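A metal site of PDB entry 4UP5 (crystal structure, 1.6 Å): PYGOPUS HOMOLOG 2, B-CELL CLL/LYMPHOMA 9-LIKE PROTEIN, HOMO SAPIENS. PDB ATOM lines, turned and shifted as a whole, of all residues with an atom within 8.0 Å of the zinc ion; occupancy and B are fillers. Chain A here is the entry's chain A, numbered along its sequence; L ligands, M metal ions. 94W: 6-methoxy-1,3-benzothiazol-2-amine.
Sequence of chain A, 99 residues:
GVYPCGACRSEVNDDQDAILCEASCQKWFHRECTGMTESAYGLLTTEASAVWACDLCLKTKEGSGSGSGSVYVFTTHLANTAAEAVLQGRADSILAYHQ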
ATOM      1  N   GLY A   6      -5.504 -20.473 -10.828  1.00  0.00           N
ATOM      2  CA  GLY A   6      -5.955 -19.736 -11.974  1.00  0.00           C
ATOM      3  C   GLY A   6      -5.553 -20.230 -13.330  1.00  0.00           C
ATOM      4  O   GLY A   6      -6.202 -19.952 -14.350  1.00  0.00           O
ATOM      5  N   LEU A  20      -1.070 -14.583  -5.418  1.00  0.00           N
ATOM      6  CA  LEU A  20      -2.415 -14.073  -5.634  1.00  0.00           C
ATOM      7  C   LEU A  20      -2.441 -12.884  -6.633  1.00  0.00           C
ATOM      8  O   LEU A  20      -1.615 -11.914  -6.525  1.00  0.00           O
ATOM      9  CB  LEU A  20      -2.853 -13.492  -4.292  1.00  0.00           C
ATOM     10  CG  LEU A  20      -4.253 -12.884  -4.299  1.00  0.00           C
ATOM     11  CD1 LEU A  20      -5.318 -13.870  -4.591  1.00  0.00           C
ATOM     12  CD2 LEU A  20      -4.475 -12.248  -2.916  1.00  0.00           C
ATOM     13  N   CYS A  21      -3.338 -12.964  -7.615  1.00  0.00           N
ATOM     14  CA  CYS A  21      -3.543 -11.898  -8.549  1.00  0.00           C
ATOM     15  C   CYS A  21      -4.332 -10.763  -7.862  1.00  0.00           C
ATOM     16  O   CYS A  21      -5.539 -10.783  -7.813  1.00  0.00           O
ATOM     17  CB  CYS A  21      -4.224 -12.318  -9.807  1.00  0.00           C
ATOM     18  SG  CYS A  21      -4.469 -10.952 -10.994  1.00  0.00           S
ATOM     19  N   GLU A  22      -3.626  -9.889  -7.212  1.00  0.00           N
ATOM     20  CA  GLU A  22      -4.250  -8.793  -6.499  1.00  0.00           C
ATOM     21  C   GLU A  22      -4.480  -7.655  -7.395  1.00  0.00           C
ATOM     22  O   GLU A  22      -5.066  -6.667  -6.981  1.00  0.00           O
ATOM     23  CB  GLU A  22      -3.371  -8.275  -5.410  1.00  0.00           C
ATOM     24  CG  GLU A  22      -3.214  -9.260  -4.310  1.00  0.00           C
ATOM     25  CD  GLU A  22      -2.368  -8.752  -3.174  1.00  0.00           C
ATOM     26  OE1 GLU A  22      -2.955  -8.077  -2.265  1.00  0.00           O
ATOM     27  OE2 GLU A  22      -1.134  -9.050  -3.156  1.00  0.00           O
ATOM     28  N   ALA A  23      -3.978  -7.709  -8.614  1.00  0.00           N
ATOM     29  CA  ALA A  23      -4.227  -6.620  -9.542  1.00  0.00           C
ATOM     30  C   ALA A  23      -5.690  -6.599  -9.845  1.00  0.00           C
ATOM     31  O   ALA A  23      -6.295  -5.524 -10.034  1.00  0.00           O
ATOM     32  CB  ALA A  23      -3.423  -6.794 -10.840  1.00  0.00           C
ATOM     33  N   SER A  24      -6.323  -7.775  -9.843  1.00  0.00           N
ATOM     34  CA  SER A  24      -7.707  -7.802 -10.208  1.00  0.00           C
ATOM     35  C   SER A  24      -8.517  -9.041  -9.863  1.00  0.00           C
ATOM     36  O   SER A  24      -9.434  -8.930  -9.057  1.00  0.00           O
ATOM     37  CB  SER A  24      -7.848  -7.576 -11.701  1.00  0.00           C
ATOM     38  OG  SER A  24      -9.237  -7.611 -12.071  1.00  0.00           O
ATOM     39  N   CYS A  25      -8.246 -10.197 -10.524  1.00  0.00           N
ATOM     40  CA  CYS A  25      -9.187 -11.324 -10.472  1.00  0.00           C
ATOM     41  C   CYS A  25      -9.227 -12.039  -9.109  1.00  0.00           C
ATOM     42  O   CYS A  25     -10.158 -12.836  -8.833  1.00  0.00           O
ATOM     43  CB  CYS A  25      -8.913 -12.322 -11.600  1.00  0.00           C
ATOM     44  SG  CYS A  25      -7.333 -13.281 -11.371  1.00  0.00           S
ATOM     45  N   GLN A  26      -8.225 -11.757  -8.287  1.00  0.00           N
ATOM     46  CA  GLN A  26      -8.107 -12.243  -6.967  1.00  0.00           C
ATOM     47  C   GLN A  26      -8.110 -13.782  -6.960  1.00  0.00           C
ATOM     48  O   GLN A  26      -8.617 -14.400  -5.961  1.00  0.00           O
ATOM     49  CB  GLN A  26      -9.302 -11.767  -6.090  1.00  0.00           C
ATOM     50  CG  GLN A  26      -9.427 -10.238  -6.006  1.00  0.00           C
ATOM     51  CD  GLN A  26      -8.132  -9.597  -5.549  1.00  0.00           C
ATOM     52  OE1 GLN A  26      -7.675  -8.616  -6.153  1.00  0.00           O
ATOM     53  NE2 GLN A  26      -7.533 -10.133  -4.499  1.00  0.00           N
ATOM     54  N   LYS A  27      -7.562 -14.381  -8.029  1.00  0.00           N
ATOM     55  CA  LYS A  27      -7.288 -15.835  -8.059  1.00  0.00           C
ATOM     56  C   LYS A  27      -5.867 -16.158  -7.667  1.00  0.00           C
ATOM     57  O   LYS A  27      -4.963 -15.348  -7.940  1.00  0.00           O
ATOM     58  CB  LYS A  27      -7.523 -16.413  -9.432  1.00  0.00           C
ATOM     59  CG  LYS A  27      -8.999 -16.409  -9.758  1.00  0.00           C
ATOM     60  CD  LYS A  27      -9.337 -16.738 -11.168  1.00  0.00           C
ATOM     61  CE  LYS A  27     -10.847 -16.519 -11.319  1.00  0.00           C
ATOM     62  NZ  LYS A  27     -11.414 -17.387 -12.374  1.00  0.00           N
ATOM     63  N   TRP A  28      -5.683 -17.317  -7.021  1.00  0.00           N
ATOM     64  CA  TRP A  28      -4.362 -17.816  -6.536  1.00  0.00           C
ATOM     65  C   TRP A  28      -3.849 -18.630  -7.697  1.00  0.00           C
ATOM     66  O   TRP A  28      -4.601 -19.340  -8.389  1.00  0.00           O
ATOM     67  CB  TRP A  28      -4.487 -18.701  -5.306  1.00  0.00           C
ATOM     68  CG  TRP A  28      -4.611 -17.926  -4.061  1.00  0.00           C
ATOM     69  CD1 TRP A  28      -5.809 -17.513  -3.451  1.00  0.00           C
ATOM     70  CD2 TRP A  28      -3.562 -17.334  -3.322  1.00  0.00           C
ATOM     71  NE1 TRP A  28      -5.512 -16.790  -2.335  1.00  0.00           N
ATOM     72  CE2 TRP A  28      -4.158 -16.640  -2.229  1.00  0.00           C
ATOM     73  CE3 TRP A  28      -2.166 -17.377  -3.412  1.00  0.00           C
ATOM     74  CZ2 TRP A  28      -3.418 -15.973  -1.298  1.00  0.00           C
ATOM     75  CZ3 TRP A  28      -1.398 -16.685  -2.462  1.00  0.00           C
ATOM     76  CH2 TRP A  28      -2.044 -16.014  -1.391  1.00  0.00           C
ATOM     77  N   PHE A  29      -2.498 -18.589  -7.851  1.00  0.00           N
ATOM     78  CA  PHE A  29      -1.876 -19.382  -8.880  1.00  0.00           C
ATOM     79  C   PHE A  29      -0.652 -20.119  -8.289  1.00  0.00           C
ATOM     80  O   PHE A  29       0.109 -19.558  -7.461  1.00  0.00           O
ATOM     81  CB  PHE A  29      -1.324 -18.471  -9.996  1.00  0.00           C
ATOM     82  CG  PHE A  29      -2.362 -17.878 -10.907  1.00  0.00           C
ATOM     83  CD1 PHE A  29      -3.193 -16.895 -10.440  1.00  0.00           C
ATOM     84  CD2 PHE A  29      -2.414 -18.246 -12.237  1.00  0.00           C
ATOM     85  CE1 PHE A  29      -4.141 -16.324 -11.280  1.00  0.00           C
ATOM     86  CE2 PHE A  29      -3.363 -17.699 -13.080  1.00  0.00           C
ATOM     87  CZ  PHE A  29      -4.195 -16.690 -12.552  1.00  0.00           C
ATOM     88  N   TRP A  52       0.947  -8.490  -7.869  1.00  0.00           N
ATOM     89  CA  TRP A  52       1.130  -9.273  -9.075  1.00  0.00           C
ATOM     90  C   TRP A  52      -0.172  -9.288  -9.861  1.00  0.00           C
ATOM     91  O   TRP A  52      -1.246  -9.315  -9.251  1.00  0.00           O
ATOM     92  CB  TRP A  52       1.590 -10.685  -8.670  1.00  0.00           C
ATOM     93  CG  TRP A  52       1.741 -11.566  -9.820  1.00  0.00           C
ATOM     94  CD1 TRP A  52       2.727 -11.535 -10.743  1.00  0.00           C
ATOM     95  CD2 TRP A  52       0.889 -12.656 -10.151  1.00  0.00           C
ATOM     96  NE1 TRP A  52       2.524 -12.514 -11.701  1.00  0.00           N
ATOM     97  CE2 TRP A  52       1.395 -13.210 -11.351  1.00  0.00           C
ATOM     98  CE3 TRP A  52      -0.293 -13.206  -9.587  1.00  0.00           C
ATOM     99  CZ2 TRP A  52       0.789 -14.336 -11.978  1.00  0.00           C
ATOM    100  CZ3 TRP A  52      -0.874 -14.271 -10.187  1.00  0.00           C
ATOM    101  CH2 TRP A  52      -0.358 -14.824 -11.397  1.00  0.00           C
ATOM    102  N   ALA A  53      -0.042  -9.202 -11.172  1.00  0.00           N
ATOM    103  CA  ALA A  53      -1.131  -9.360 -12.101  1.00  0.00           C
ATOM    104  C   ALA A  53      -0.905 -10.566 -12.971  1.00  0.00           C
ATOM    105  O   ALA A  53       0.189 -10.723 -13.567  1.00  0.00           O
ATOM    106  CB  ALA A  53      -1.198  -8.132 -12.979  1.00  0.00           C
ATOM    107  N   CYS A  54      -1.921 -11.421 -13.078  1.00  0.00           N
ATOM    108  CA  CYS A  54      -1.881 -12.544 -13.964  1.00  0.00           C
ATOM    109  C   CYS A  54      -2.019 -12.150 -15.409  1.00  0.00           C
ATOM    110  O   CYS A  54      -2.339 -10.962 -15.687  1.00  0.00           O
ATOM    111  CB  CYS A  54      -2.863 -13.623 -13.578  1.00  0.00           C
ATOM    112  SG  CYS A  54      -4.558 -13.204 -14.166  1.00  0.00           S
ATOM    113  N   ASP A  55      -1.688 -13.081 -16.305  1.00  0.00           N
ATOM    114  CA  ASP A  55      -1.697 -12.805 -17.773  1.00  0.00           C
ATOM    115  C   ASP A  55      -3.071 -12.332 -18.293  1.00  0.00           C
ATOM    116  O   ASP A  55      -3.143 -11.664 -19.317  1.00  0.00           O
ATOM    117  CB  ASP A  55      -1.232 -14.010 -18.561  1.00  0.00           C
ATOM    118  CG  ASP A  55       0.276 -14.234 -18.482  1.00  0.00           C
ATOM    119  OD1 ASP A  55       1.091 -13.346 -17.994  1.00  0.00           O
ATOM    120  OD2 ASP A  55       0.651 -15.343 -18.904  1.00  0.00           O
ATOM    121  N   LEU A  56      -4.139 -12.643 -17.565  1.00  0.00           N
ATOM    122  CA  LEU A  56      -5.461 -12.175 -17.941  1.00  0.00           C
ATOM    123  C   LEU A  56      -5.770 -10.819 -17.403  1.00  0.00           C
ATOM    124  O   LEU A  56      -6.483 -10.090 -18.049  1.00  0.00           O
ATOM    125  CB  LEU A  56      -6.484 -13.210 -17.524  1.00  0.00           C
ATOM    126  CG  LEU A  56      -6.312 -14.571 -18.212  1.00  0.00           C
ATOM    127  CD1 LEU A  56      -7.506 -15.442 -17.844  1.00  0.00           C
ATOM    128  CD2 LEU A  56      -6.221 -14.415 -19.734  1.00  0.00           C
ATOM    129  N   CYS A  57      -5.188 -10.393 -16.307  1.00  0.00           N
ATOM    130  CA  CYS A  57      -5.544  -9.116 -15.729  1.00  0.00           C
ATOM    131  C   CYS A  57      -4.626  -7.941 -16.198  1.00  0.00           C
ATOM    132  O   CYS A  57      -3.729  -8.145 -17.048  1.00  0.00           O
ATOM    133  CB  CYS A  57      -5.588  -9.258 -14.250  1.00  0.00           C
ATOM    134  SG  CYS A  57      -6.947 -10.367 -13.776  1.00  0.00           S
HETATM  135  C01 94W L   1      -3.485 -18.610 -17.455  1.00  0.00           C
HETATM  136  O02 94W L   1      -4.297 -19.554 -18.045  1.00  0.00           O
HETATM  137  C03 94W L   1      -3.995 -20.918 -17.811  1.00  0.00           C
HETATM  138  C04 94W L   1      -2.119 -18.800 -17.460  1.00  0.00           C
HETATM  139  C05 94W L   1      -1.329 -17.840 -16.853  1.00  0.00           C
HETATM  140  C06 94W L   1      -1.880 -16.705 -16.246  1.00  0.00           C
HETATM  141  C07 94W L   1      -3.264 -16.546 -16.261  1.00  0.00           C
HETATM  142  C08 94W L   1      -4.063 -17.501 -16.867  1.00  0.00           C
HETATM  143  N09 94W L   1      -0.965 -15.819 -15.685  1.00  0.00           N
HETATM  144  C10 94W L   1       0.258 -16.263 -15.844  1.00  0.00           C
HETATM  145  N11 94W L   1       1.351 -15.636 -15.403  1.00  0.00           N
HETATM  146  S12 94W L   1       0.408 -17.794 -16.702  1.00  0.00           S
HETATM  147 ZN    ZN M   1      -5.820 -11.961 -12.573  1.00  0.00          ZN
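Within 4 Å of the zinc ion: Cys 21, Cys 25, Cys 54 and Cys 57.
The zinc ion is bound by SG of Cys 57 (2.3 Å), SG of Cys 21 (2.3 Å), SG of Cys 25 (2.3 Å) and SG of Cys 54 (2.4 Å). The zinc ion has four donor atoms within binding distance.
The backbone NH (N) of Asp 55 lies within hydrogen-bond range of a nitrogen (N09) of the ligand (2.9 Å). OD1 of Asp 55 is in hydrogen-bond range of N11 of the ligand (3.5 Å).
The backbone NH (N) of Gln 26 lies within hydrogen-bond range of the backbone carbonyl oxygen (O) of Cys 21 (2.9 Å). The backbone carbonyl oxygen of Lys 27 lies within hydrogen-bond range of the backbone NH of Cys 21 (2.9 Å). The side-chain sulfur (SG) of Cys 25 lies close to the backbone NH (N) of Lys 27, at 3.5 Å. The backbone NH (N) of Leu 56 lies close to the side-chain sulfur (SG) of Cys 54, 3.5 Å away.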
